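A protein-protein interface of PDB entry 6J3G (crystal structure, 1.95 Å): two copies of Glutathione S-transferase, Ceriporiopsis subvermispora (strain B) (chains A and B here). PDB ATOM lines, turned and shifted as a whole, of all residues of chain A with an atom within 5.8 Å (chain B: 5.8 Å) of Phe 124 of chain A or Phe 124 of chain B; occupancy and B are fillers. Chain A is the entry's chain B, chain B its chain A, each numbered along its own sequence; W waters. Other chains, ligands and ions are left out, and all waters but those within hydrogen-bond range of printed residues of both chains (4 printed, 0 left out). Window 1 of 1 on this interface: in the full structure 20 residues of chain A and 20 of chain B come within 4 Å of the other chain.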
ATOM      1  N   GLU A 120     -21.812  15.430   4.034  1.00  0.00           N
ATOM      2  CA  GLU A 120     -22.495  15.145   2.776  1.00  0.00           C
ATOM      3  C   GLU A 120     -22.262  16.224   1.724  1.00  0.00           C
ATOM      4  O   GLU A 120     -22.584  16.002   0.552  1.00  0.00           O
ATOM      5  CB  GLU A 120     -24.001  14.980   3.025  1.00  0.00           C
ATOM      6  CG  GLU A 120     -24.575  16.037   3.962  1.00  0.00           C
ATOM      7  CD  GLU A 120     -24.626  15.621   5.439  1.00  0.00           C
ATOM      8  OE1 GLU A 120     -25.712  15.758   6.048  1.00  0.00           O
ATOM      9  OE2 GLU A 120     -23.593  15.187   6.003  1.00  0.00           O
ATOM     10  N   LEU A 121     -21.718  17.383   2.106  1.00  0.00           N
ATOM     11  CA  LEU A 121     -21.423  18.445   1.152  1.00  0.00           C
ATOM     12  C   LEU A 121     -20.017  18.355   0.553  1.00  0.00           C
ATOM     13  O   LEU A 121     -19.761  18.978  -0.484  1.00  0.00           O
ATOM     14  CB  LEU A 121     -21.593  19.807   1.836  1.00  0.00           C
ATOM     15  CG  LEU A 121     -21.243  21.084   1.078  1.00  0.00           C
ATOM     16  CD1 LEU A 121     -22.136  21.241  -0.147  1.00  0.00           C
ATOM     17  CD2 LEU A 121     -21.385  22.301   1.999  1.00  0.00           C
ATOM     18  N   GLU A 122     -19.108  17.603   1.181  1.00  0.00           N
ATOM     19  CA  GLU A 122     -17.677  17.777   0.927  1.00  0.00           C
ATOM     20  C   GLU A 122     -17.309  17.500  -0.530  1.00  0.00           C
ATOM     21  O   GLU A 122     -16.546  18.259  -1.141  1.00  0.00           O
ATOM     22  CB  GLU A 122     -16.866  16.875   1.859  1.00  0.00           C
ATOM     23  CG  GLU A 122     -16.819  17.354   3.314  1.00  0.00           C
ATOM     24  CD  GLU A 122     -15.674  18.316   3.595  1.00  0.00           C
ATOM     25  OE1 GLU A 122     -14.985  18.734   2.638  1.00  0.00           O
ATOM     26  OE2 GLU A 122     -15.450  18.641   4.781  1.00  0.00           O
ATOM     27  N   ALA A 123     -17.811  16.401  -1.101  1.00  0.00           N
ATOM     28  CA  ALA A 123     -17.438  16.081  -2.479  1.00  0.00           C
ATOM     29  C   ALA A 123     -18.077  17.059  -3.454  1.00  0.00           C
ATOM     30  O   ALA A 123     -17.416  17.559  -4.371  1.00  0.00           O
ATOM     31  CB  ALA A 123     -17.832  14.639  -2.821  1.00  0.00           C
ATOM     32  N   PHE A 124     -19.354  17.370  -3.252  1.00  0.00           N
ATOM     33  CA  PHE A 124     -20.022  18.278  -4.169  1.00  0.00           C
ATOM     34  C   PHE A 124     -19.451  19.684  -4.080  1.00  0.00           C
ATOM     35  O   PHE A 124     -19.454  20.413  -5.078  1.00  0.00           O
ATOM     36  CB  PHE A 124     -21.523  18.307  -3.883  1.00  0.00           C
ATOM     37  CG  PHE A 124     -22.255  17.134  -4.447  1.00  0.00           C
ATOM     38  CD1 PHE A 124     -22.310  16.931  -5.816  1.00  0.00           C
ATOM     39  CD2 PHE A 124     -22.891  16.235  -3.609  1.00  0.00           C
ATOM     40  CE1 PHE A 124     -22.996  15.839  -6.343  1.00  0.00           C
ATOM     41  CE2 PHE A 124     -23.576  15.141  -4.134  1.00  0.00           C
ATOM     42  CZ  PHE A 124     -23.615  14.950  -5.496  1.00  0.00           C
ATOM     43  N   HIS A 125     -18.977  20.096  -2.904  1.00  0.00           N
ATOM     44  CA  HIS A 125     -18.382  21.422  -2.838  1.00  0.00           C
ATOM     45  C   HIS A 125     -17.024  21.450  -3.528  1.00  0.00           C
ATOM     46  O   HIS A 125     -16.655  22.459  -4.141  1.00  0.00           O
ATOM     47  CB  HIS A 125     -18.239  21.918  -1.399  1.00  0.00           C
ATOM     48  CG  HIS A 125     -17.570  23.251  -1.346  1.00  0.00           C
ATOM     49  ND1 HIS A 125     -18.230  24.416  -1.665  1.00  0.00           N
ATOM     50  CD2 HIS A 125     -16.271  23.592  -1.156  1.00  0.00           C
ATOM     51  CE1 HIS A 125     -17.379  25.428  -1.623  1.00  0.00           C
ATOM     52  NE2 HIS A 125     -16.182  24.952  -1.328  1.00  0.00           N
ATOM     53  N   ALA A 126     -16.270  20.354  -3.435  1.00  0.00           N
ATOM     54  CA  ALA A 126     -15.038  20.220  -4.204  1.00  0.00           C
ATOM     55  C   ALA A 126     -15.311  20.269  -5.702  1.00  0.00           C
ATOM     56  O   ALA A 126     -14.559  20.899  -6.456  1.00  0.00           O
ATOM     57  CB  ALA A 126     -14.331  18.915  -3.836  1.00  0.00           C
ATOM     58  N   VAL A 127     -16.360  19.573  -6.156  1.00  0.00           N
ATOM     59  CA  VAL A 127     -16.802  19.713  -7.543  1.00  0.00           C
ATOM     60  C   VAL A 127     -17.033  21.180  -7.871  1.00  0.00           C
ATOM     61  O   VAL A 127     -16.515  21.711  -8.861  1.00  0.00           O
ATOM     62  CB  VAL A 127     -18.090  18.906  -7.790  1.00  0.00           C
ATOM     63  CG1 VAL A 127     -18.585  19.182  -9.215  1.00  0.00           C
ATOM     64  CG2 VAL A 127     -17.874  17.412  -7.560  1.00  0.00           C
ATOM     65  N   PHE A 128     -17.835  21.850  -7.039  1.00  0.00           N
ATOM     66  CA  PHE A 128     -18.145  23.260  -7.252  1.00  0.00           C
ATOM     67  C   PHE A 128     -16.878  24.128  -7.367  1.00  0.00           C
ATOM     68  O   PHE A 128     -16.791  24.991  -8.248  1.00  0.00           O
ATOM     69  CB  PHE A 128     -19.062  23.756  -6.124  1.00  0.00           C
ATOM     70  CG  PHE A 128     -19.089  25.250  -5.988  1.00  0.00           C
ATOM     71  CD1 PHE A 128     -19.977  26.012  -6.729  1.00  0.00           C
ATOM     72  CD2 PHE A 128     -18.209  25.893  -5.122  1.00  0.00           C
ATOM     73  CE1 PHE A 128     -19.991  27.401  -6.609  1.00  0.00           C
ATOM     74  CE2 PHE A 128     -18.211  27.270  -5.005  1.00  0.00           C
ATOM     75  CZ  PHE A 128     -19.102  28.025  -5.747  1.00  0.00           C
ATOM     76  N   GLU A 129     -15.885  23.937  -6.487  1.00  0.00           N
ATOM     77  CA  GLU A 129     -14.705  24.804  -6.572  1.00  0.00           C
ATOM     78  C   GLU A 129     -14.044  24.714  -7.947  1.00  0.00           C
ATOM     79  O   GLU A 129     -13.553  25.720  -8.479  1.00  0.00           O
ATOM     80  CB  GLU A 129     -13.690  24.465  -5.473  1.00  0.00           C
ATOM     81  CG  GLU A 129     -14.169  24.758  -4.052  1.00  0.00           C
ATOM     82  CD  GLU A 129     -14.025  26.226  -3.648  1.00  0.00           C
ATOM     83  OE1 GLU A 129     -14.326  26.539  -2.479  1.00  0.00           O
ATOM     84  OE2 GLU A 129     -13.605  27.066  -4.478  1.00  0.00           O
ATOM     85  N   TRP A 203     -27.235  26.718 -12.719  1.00  0.00           N
ATOM     86  CA  TRP A 203     -27.110  25.617 -11.767  1.00  0.00           C
ATOM     87  C   TRP A 203     -28.184  25.718 -10.698  1.00  0.00           C
ATOM     88  O   TRP A 203     -28.834  24.726 -10.343  1.00  0.00           O
ATOM     89  CB  TRP A 203     -25.729  25.615 -11.101  1.00  0.00           C
ATOM     90  CG  TRP A 203     -24.581  25.495 -12.033  1.00  0.00           C
ATOM     91  CD1 TRP A 203     -24.577  24.898 -13.256  1.00  0.00           C
ATOM     92  CD2 TRP A 203     -23.249  25.982 -11.813  1.00  0.00           C
ATOM     93  NE1 TRP A 203     -23.319  24.986 -13.819  1.00  0.00           N
ATOM     94  CE2 TRP A 203     -22.491  25.654 -12.953  1.00  0.00           C
ATOM     95  CE3 TRP A 203     -22.632  26.679 -10.767  1.00  0.00           C
ATOM     96  CZ2 TRP A 203     -21.138  25.992 -13.077  1.00  0.00           C
ATOM     97  CZ3 TRP A 203     -21.290  27.002 -10.884  1.00  0.00           C
ATOM     98  CH2 TRP A 203     -20.558  26.668 -12.036  1.00  0.00           C
ATOM     99  N   PHE A 214     -27.760  26.889  -2.746  1.00  0.00           N
ATOM    100  CA  PHE A 214     -27.501  25.656  -3.484  1.00  0.00           C
ATOM    101  C   PHE A 214     -28.309  24.476  -2.954  1.00  0.00           C
ATOM    102  O   PHE A 214     -28.871  23.698  -3.740  1.00  0.00           O
ATOM    103  CB  PHE A 214     -26.007  25.347  -3.468  1.00  0.00           C
ATOM    104  CG  PHE A 214     -25.255  26.101  -4.513  1.00  0.00           C
ATOM    105  CD1 PHE A 214     -24.749  27.368  -4.242  1.00  0.00           C
ATOM    106  CD2 PHE A 214     -25.092  25.574  -5.780  1.00  0.00           C
ATOM    107  CE1 PHE A 214     -24.071  28.083  -5.213  1.00  0.00           C
ATOM    108  CE2 PHE A 214     -24.410  26.283  -6.753  1.00  0.00           C
ATOM    109  CZ  PHE A 214     -23.904  27.543  -6.469  1.00  0.00           C
ATOM    110  N   MET A 215     -28.391  24.320  -1.638  1.00  0.00           N
ATOM    111  CA  MET A 215     -29.140  23.178  -1.124  1.00  0.00           C
ATOM    112  C   MET A 215     -30.649  23.388  -1.130  1.00  0.00           C
ATOM    113  O   MET A 215     -31.392  22.418  -0.927  1.00  0.00           O
ATOM    114  CB  MET A 215     -28.641  22.828   0.276  1.00  0.00           C
ATOM    115  CG  MET A 215     -27.302  22.065   0.187  1.00  0.00           C
ATOM    116  SD  MET A 215     -26.694  21.466   1.748  1.00  0.00           S
ATOM    117  CE  MET A 215     -27.154  22.854   2.718  1.00  0.00           C
ATOM    118  N   CYS A 220     -25.221  27.188   2.863  1.00  0.00           N
ATOM    119  CA  CYS A 220     -24.084  26.364   3.263  1.00  0.00           C
ATOM    120  C   CYS A 220     -22.803  27.042   2.799  1.00  0.00           C
ATOM    121  O   CYS A 220     -22.828  28.155   2.266  1.00  0.00           O
ATOM    122  CB  CYS A 220     -24.207  24.932   2.718  1.00  0.00           C
ATOM    123  SG  CYS A 220     -23.909  24.741   0.950  1.00  0.00           S
ATOM    124  N   THR A 222     -20.924  26.679   0.294  1.00  0.00           N
ATOM    125  CA  THR A 222     -20.678  27.073  -1.088  1.00  0.00           C
ATOM    126  C   THR A 222     -21.417  28.369  -1.432  1.00  0.00           C
ATOM    127  O   THR A 222     -20.895  29.175  -2.210  1.00  0.00           O
ATOM    128  CB  THR A 222     -20.942  25.896  -2.069  1.00  0.00           C
ATOM    129  OG1 THR A 222     -21.802  26.243  -3.153  1.00  0.00           O
ATOM    130  CG2 THR A 222     -21.378  24.629  -1.390  1.00  0.00           C
ATOM    131  N   GLU B 120     -32.603  18.414  -3.013  1.00  0.00           N
ATOM    132  CA  GLU B 120     -31.370  19.002  -2.506  1.00  0.00           C
ATOM    133  C   GLU B 120     -30.152  18.624  -3.343  1.00  0.00           C
ATOM    134  O   GLU B 120     -29.084  19.210  -3.144  1.00  0.00           O
ATOM    135  CB  GLU B 120     -31.165  18.616  -1.039  1.00  0.00           C
ATOM    136  CG  GLU B 120     -31.069  17.118  -0.767  1.00  0.00           C
ATOM    137  CD  GLU B 120     -32.421  16.429  -0.512  1.00  0.00           C
ATOM    138  OE1 GLU B 120     -33.496  17.019  -0.793  1.00  0.00           O
ATOM    139  OE2 GLU B 120     -32.395  15.275  -0.021  1.00  0.00           O
ATOM    140  N   LEU B 121     -30.288  17.695  -4.293  1.00  0.00           N
ATOM    141  CA  LEU B 121     -29.188  17.379  -5.202  1.00  0.00           C
ATOM    142  C   LEU B 121     -29.200  18.224  -6.477  1.00  0.00           C
ATOM    143  O   LEU B 121     -28.163  18.332  -7.148  1.00  0.00           O
ATOM    144  CB  LEU B 121     -29.229  15.883  -5.563  1.00  0.00           C
ATOM    145  CG  LEU B 121     -28.261  15.336  -6.623  1.00  0.00           C
ATOM    146  CD1 LEU B 121     -26.838  15.504  -6.147  1.00  0.00           C
ATOM    147  CD2 LEU B 121     -28.547  13.866  -6.937  1.00  0.00           C
ATOM    148  N   GLU B 122     -30.327  18.862  -6.808  1.00  0.00           N
ATOM    149  CA  GLU B 122     -30.535  19.348  -8.176  1.00  0.00           C
ATOM    150  C   GLU B 122     -29.479  20.360  -8.597  1.00  0.00           C
ATOM    151  O   GLU B 122     -28.927  20.265  -9.701  1.00  0.00           O
ATOM    152  CB  GLU B 122     -31.932  19.949  -8.319  1.00  0.00           C
ATOM    153  CG  GLU B 122     -33.028  18.898  -8.354  1.00  0.00           C
ATOM    154  CD  GLU B 122     -33.290  18.377  -9.762  1.00  0.00           C
ATOM    155  OE1 GLU B 122     -32.512  18.695 -10.697  1.00  0.00           O
ATOM    156  OE2 GLU B 122     -34.292  17.663  -9.936  1.00  0.00           O
ATOM    157  N   ALA B 123     -29.194  21.351  -7.745  1.00  0.00           N
ATOM    158  CA  ALA B 123     -28.226  22.378  -8.123  1.00  0.00           C
ATOM    159  C   ALA B 123     -26.804  21.827  -8.134  1.00  0.00           C
ATOM    160  O   ALA B 123     -26.043  22.094  -9.070  1.00  0.00           O
ATOM    161  CB  ALA B 123     -28.327  23.594  -7.187  1.00  0.00           C
ATOM    162  N   PHE B 124     -26.429  21.036  -7.118  1.00  0.00           N
ATOM    163  CA  PHE B 124     -25.076  20.483  -7.110  1.00  0.00           C
ATOM    164  C   PHE B 124     -24.873  19.487  -8.237  1.00  0.00           C
ATOM    165  O   PHE B 124     -23.750  19.355  -8.748  1.00  0.00           O
ATOM    166  CB  PHE B 124     -24.757  19.811  -5.775  1.00  0.00           C
ATOM    167  CG  PHE B 124     -24.454  20.781  -4.682  1.00  0.00           C
ATOM    168  CD1 PHE B 124     -23.320  21.577  -4.752  1.00  0.00           C
ATOM    169  CD2 PHE B 124     -25.311  20.926  -3.610  1.00  0.00           C
ATOM    170  CE1 PHE B 124     -23.048  22.493  -3.770  1.00  0.00           C
ATOM    171  CE2 PHE B 124     -25.032  21.854  -2.610  1.00  0.00           C
ATOM    172  CZ  PHE B 124     -23.900  22.629  -2.699  1.00  0.00           C
ATOM    173  N   HIS B 125     -25.925  18.762  -8.636  1.00  0.00           N
ATOM    174  CA  HIS B 125     -25.736  17.877  -9.775  1.00  0.00           C
ATOM    175  C   HIS B 125     -25.575  18.675 -11.064  1.00  0.00           C
ATOM    176  O   HIS B 125     -24.800  18.285 -11.948  1.00  0.00           O
ATOM    177  CB  HIS B 125     -26.875  16.869  -9.931  1.00  0.00           C
ATOM    178  CG  HIS B 125     -26.674  15.998 -11.131  1.00  0.00           C
ATOM    179  ND1 HIS B 125     -25.798  14.937 -11.127  1.00  0.00           N
ATOM    180  CD2 HIS B 125     -27.133  16.105 -12.400  1.00  0.00           C
ATOM    181  CE1 HIS B 125     -25.760  14.394 -12.333  1.00  0.00           C
ATOM    182  NE2 HIS B 125     -26.551  15.091 -13.125  1.00  0.00           N
ATOM    183  N   ALA B 126     -26.290  19.793 -11.194  1.00  0.00           N
ATOM    184  CA  ALA B 126     -26.083  20.654 -12.354  1.00  0.00           C
ATOM    185  C   ALA B 126     -24.654  21.193 -12.385  1.00  0.00           C
ATOM    186  O   ALA B 126     -24.035  21.277 -13.453  1.00  0.00           O
ATOM    187  CB  ALA B 126     -27.093  21.804 -12.344  1.00  0.00           C
ATOM    188  N   VAL B 127     -24.115  21.567 -11.218  1.00  0.00           N
ATOM    189  CA  VAL B 127     -22.711  21.969 -11.147  1.00  0.00           C
ATOM    190  C   VAL B 127     -21.817  20.835 -11.640  1.00  0.00           C
ATOM    191  O   VAL B 127     -20.903  21.043 -12.444  1.00  0.00           O
ATOM    192  CB  VAL B 127     -22.339  22.382  -9.712  1.00  0.00           C
ATOM    193  CG1 VAL B 127     -20.841  22.690  -9.621  1.00  0.00           C
ATOM    194  CG2 VAL B 127     -23.156  23.588  -9.259  1.00  0.00           C
ATOM    195  N   PHE B 128     -22.082  19.616 -11.168  1.00  0.00           N
ATOM    196  CA  PHE B 128     -21.287  18.456 -11.566  1.00  0.00           C
ATOM    197  C   PHE B 128     -21.286  18.262 -13.079  1.00  0.00           C
ATOM    198  O   PHE B 128     -20.241  17.975 -13.675  1.00  0.00           O
ATOM    199  CB  PHE B 128     -21.820  17.197 -10.870  1.00  0.00           C
ATOM    200  CG  PHE B 128     -21.325  15.913 -11.484  1.00  0.00           C
ATOM    201  CD1 PHE B 128     -20.094  15.381 -11.125  1.00  0.00           C
ATOM    202  CD2 PHE B 128     -22.088  15.242 -12.434  1.00  0.00           C
ATOM    203  CE1 PHE B 128     -19.630  14.197 -11.712  1.00  0.00           C
ATOM    204  CE2 PHE B 128     -21.630  14.071 -13.010  1.00  0.00           C
ATOM    205  CZ  PHE B 128     -20.399  13.548 -12.645  1.00  0.00           C
ATOM    206  N   GLU B 129     -22.452  18.373 -13.720  1.00  0.00           N
ATOM    207  CA  GLU B 129     -22.490  18.120 -15.157  1.00  0.00           C
ATOM    208  C   GLU B 129     -21.567  19.072 -15.902  1.00  0.00           C
ATOM    209  O   GLU B 129     -20.885  18.667 -16.853  1.00  0.00           O
ATOM    210  CB  GLU B 129     -23.927  18.214 -15.687  1.00  0.00           C
ATOM    211  CG  GLU B 129     -24.835  17.095 -15.174  1.00  0.00           C
ATOM    212  CD  GLU B 129     -24.740  15.801 -15.983  1.00  0.00           C
ATOM    213  OE1 GLU B 129     -25.451  14.836 -15.625  1.00  0.00           O
ATOM    214  OE2 GLU B 129     -23.974  15.746 -16.975  1.00  0.00           O
ATOM    215  N   TRP B 203     -12.285  15.031  -6.000  1.00  0.00           N
ATOM    216  CA  TRP B 203     -13.554  15.523  -5.458  1.00  0.00           C
ATOM    217  C   TRP B 203     -14.088  14.574  -4.401  1.00  0.00           C
ATOM    218  O   TRP B 203     -14.525  14.994  -3.320  1.00  0.00           O
ATOM    219  CB  TRP B 203     -14.601  15.683  -6.567  1.00  0.00           C
ATOM    220  CG  TRP B 203     -14.199  16.626  -7.639  1.00  0.00           C
ATOM    221  CD1 TRP B 203     -13.340  17.683  -7.526  1.00  0.00           C
ATOM    222  CD2 TRP B 203     -14.639  16.601  -8.996  1.00  0.00           C
ATOM    223  NE1 TRP B 203     -13.224  18.326  -8.742  1.00  0.00           N
ATOM    224  CE2 TRP B 203     -14.009  17.674  -9.660  1.00  0.00           C
ATOM    225  CE3 TRP B 203     -15.517  15.779  -9.714  1.00  0.00           C
ATOM    226  CZ2 TRP B 203     -14.230  17.946 -11.018  1.00  0.00           C
ATOM    227  CZ3 TRP B 203     -15.733  16.041 -11.049  1.00  0.00           C
ATOM    228  CH2 TRP B 203     -15.092  17.116 -11.694  1.00  0.00           C
ATOM    229  N   PHE B 214     -20.772  10.075  -4.091  1.00  0.00           N
ATOM    230  CA  PHE B 214     -20.645  11.512  -3.838  1.00  0.00           C
ATOM    231  C   PHE B 214     -21.267  11.917  -2.503  1.00  0.00           C
ATOM    232  O   PHE B 214     -20.682  12.722  -1.767  1.00  0.00           O
ATOM    233  CB  PHE B 214     -21.266  12.319  -4.986  1.00  0.00           C
ATOM    234  CG  PHE B 214     -20.361  12.457  -6.171  1.00  0.00           C
ATOM    235  CD1 PHE B 214     -20.360  11.490  -7.179  1.00  0.00           C
ATOM    236  CD2 PHE B 214     -19.488  13.528  -6.272  1.00  0.00           C
ATOM    237  CE1 PHE B 214     -19.502  11.602  -8.261  1.00  0.00           C
ATOM    238  CE2 PHE B 214     -18.632  13.646  -7.354  1.00  0.00           C
ATOM    239  CZ  PHE B 214     -18.636  12.687  -8.347  1.00  0.00           C
ATOM    240  N   MET B 215     -22.458  11.391  -2.175  1.00  0.00           N
ATOM    241  CA  MET B 215     -23.096  11.773  -0.916  1.00  0.00           C
ATOM    242  C   MET B 215     -22.428  11.140   0.297  1.00  0.00           C
ATOM    243  O   MET B 215     -22.642  11.616   1.421  1.00  0.00           O
ATOM    244  CB  MET B 215     -24.578  11.394  -0.931  1.00  0.00           C
ATOM    245  CG  MET B 215     -25.459  12.352  -1.716  1.00  0.00           C
ATOM    246  SD  MET B 215     -27.116  11.666  -1.924  1.00  0.00           S
ATOM    247  CE  MET B 215     -27.968  12.998  -2.757  1.00  0.00           C
ATOM    248  N   CYS B 220     -26.395   8.119  -5.554  1.00  0.00           N
ATOM    249  CA  CYS B 220     -27.409   9.000  -6.134  1.00  0.00           C
ATOM    250  C   CYS B 220     -27.176   9.079  -7.640  1.00  0.00           C
ATOM    251  O   CYS B 220     -26.314   8.382  -8.196  1.00  0.00           O
ATOM    252  CB  CYS B 220     -27.397  10.386  -5.467  1.00  0.00           C
ATOM    253  SG  CYS B 220     -25.995  11.470  -5.898  1.00  0.00           S
ATOM    254  N   THR B 222     -25.727  11.210  -9.527  1.00  0.00           N
ATOM    255  CA  THR B 222     -24.466  11.615 -10.144  1.00  0.00           C
ATOM    256  C   THR B 222     -23.453  10.471 -10.127  1.00  0.00           C
ATOM    257  O   THR B 222     -22.657  10.365 -11.061  1.00  0.00           O
ATOM    258  CB  THR B 222     -23.936  12.942  -9.540  1.00  0.00           C
ATOM    259  OG1 THR B 222     -22.573  12.861  -9.116  1.00  0.00           O
ATOM    260  CG2 THR B 222     -24.830  13.503  -8.479  1.00  0.00           C
HETATM  261  O   HOH W   1     -20.660  15.556  -1.213  1.00  0.00           O
HETATM  262  O   HOH W   2     -33.700  21.451  -2.222  1.00  0.00           O
HETATM  263  O   HOH W   3     -28.461  21.161  -4.869  1.00  0.00           O
HETATM  264  O   HOH W   4     -21.181  12.150   3.801  1.00  0.00           O
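The side-chain sulfur of Cys 220 of chain B sits close to the backbone NH of Thr 222 of chain B, 3.6 Å away.
The backbone NH (N) of Thr 222 of chain A sits close to the side-chain sulfur (SG) of Cys 220 of chain A (3.6 Å).
Among the printed residues, pairs that only touch across the chains: Ala 123 of chain A with Trp 203 of chain B, Trp 203 of chain A with Ala 123 of chain B, Phe 124 of chain A with Leu 121 of chain B, Leu 121 of chain A with Phe 124 of chain B, Thr 222 of chain A with Phe 124 of chain B, Trp 203 of chain A with Val 127 of chain B, Phe 214 of chain A with Ala 123 of chain B, Phe 214 of chain A with Phe 124 of chain B, Phe 124 of chain A with Thr 222 of chain B, Phe 124 of chain A with Phe 214 of chain B, Val 127 of chain A with Trp 203 of chain B, Ala 123 of chain A with Phe 214 of chain B, Ala 126 of chain A with Trp 203 of chain B, Met 215 of chain A with Phe 124 of chain B, Phe 128 of chain A with Val 127 of chain B, Val 127 of chain A with Phe 128 of chain B, Trp 203 of chain A with Ala 126 of chain B, Met 215 of chain A with Glu 120 of chain B, Phe 124 of chain A with Phe 124 of chain B, Glu 120 of chain A with Met 215 of chain B, Val 127 of chain A with Phe 214 of chain B and Phe 214 of chain A with Val 127 of chain B.
Cys 220 of chain A touches none of the printed residues of chain B.
Of the printed residues of chain A, Glu 120 of chain B touches Met 215 (3.8 Å).
Of the printed residues of chain A, Leu 121 of chain B touches Phe 124.
Glu 122 of chain B touches none of the printed residues of chain A.
Phe 124 of chain B touches five residues of chain A.
Printed residues of chain A within 4 Å of Met 215 of chain B: Glu 120 (3.8 Å).
The nearest printed residue of chain B that does not touch Phe 124 of chain A is Met 215 of chain B (4.1 Å).
The nearest printed residue of chain B that does not touch Phe 214 of chain A is Glu 120 of chain B (4.5 Å).
Of the 15 printed residues of chain A, 11 touch a printed residue of chain B.
Hydrophobic or aromatic side chains of chain A within 4 Å of the printed part of chain B: Leu 121, Ala 123, Phe 124, Ala 126, Val 127, Trp 203, Phe 214 and Met 215.
Among the printed residues, 22 pairs touch across the chains.
Among the printed residues, no Asp or Glu carboxylate lies within 4 Å of a Lys or Arg side-chain nitrogen of the other chain.
Leu 121 of chain A touches Phe 124 of chain B, and with the chains exchanged Phe 124 of chain A touches Leu 121 of chain B.
Ala 123 of chain A touches Phe 214 of chain B, and with the chains exchanged Phe 214 of chain A touches Ala 123 of chain B.
Phe 124 of chain A touches its own counterpart, Phe 124 of chain B.
Val 127 of chain A touches Phe 128 of chain B, and with the chains exchanged Phe 128 of chain A touches Val 127 of chain B.
Positions printed for both chains: 120, 121, 122, 123, 124, 125, 126, 127, 128, 129, 203, 214, 215, 220 and 222.
Water W1 lies within hydrogen-bond range of the backbone carbonyl oxygen of Glu 120 of chain A, the backbone carbonyl oxygen of Phe 214 of chain B, the backbone NH of Ala 123 of chain A and the backbone NH of Phe 124 of chain A.
Water W3 lies within hydrogen-bond range of the backbone carbonyl oxygen of Glu 120 of chain B (2.7 Å), the backbone carbonyl oxygen of Phe 214 of chain A (2.8 Å), the backbone NH of Ala 123 of chain B (3.0 Å) and the backbone NH of Phe 124 of chain B (3.0 Å).
Water W2 bridges the backbone carbonyl oxygen (O) of Met 215 of chain A and the backbone NH (N) of Glu 120 of chain B.
Water W4 lies within hydrogen-bond range of the backbone carbonyl oxygen (O) of Met 215 of chain B and the backbone NH (N) of Glu 120 of chain A.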
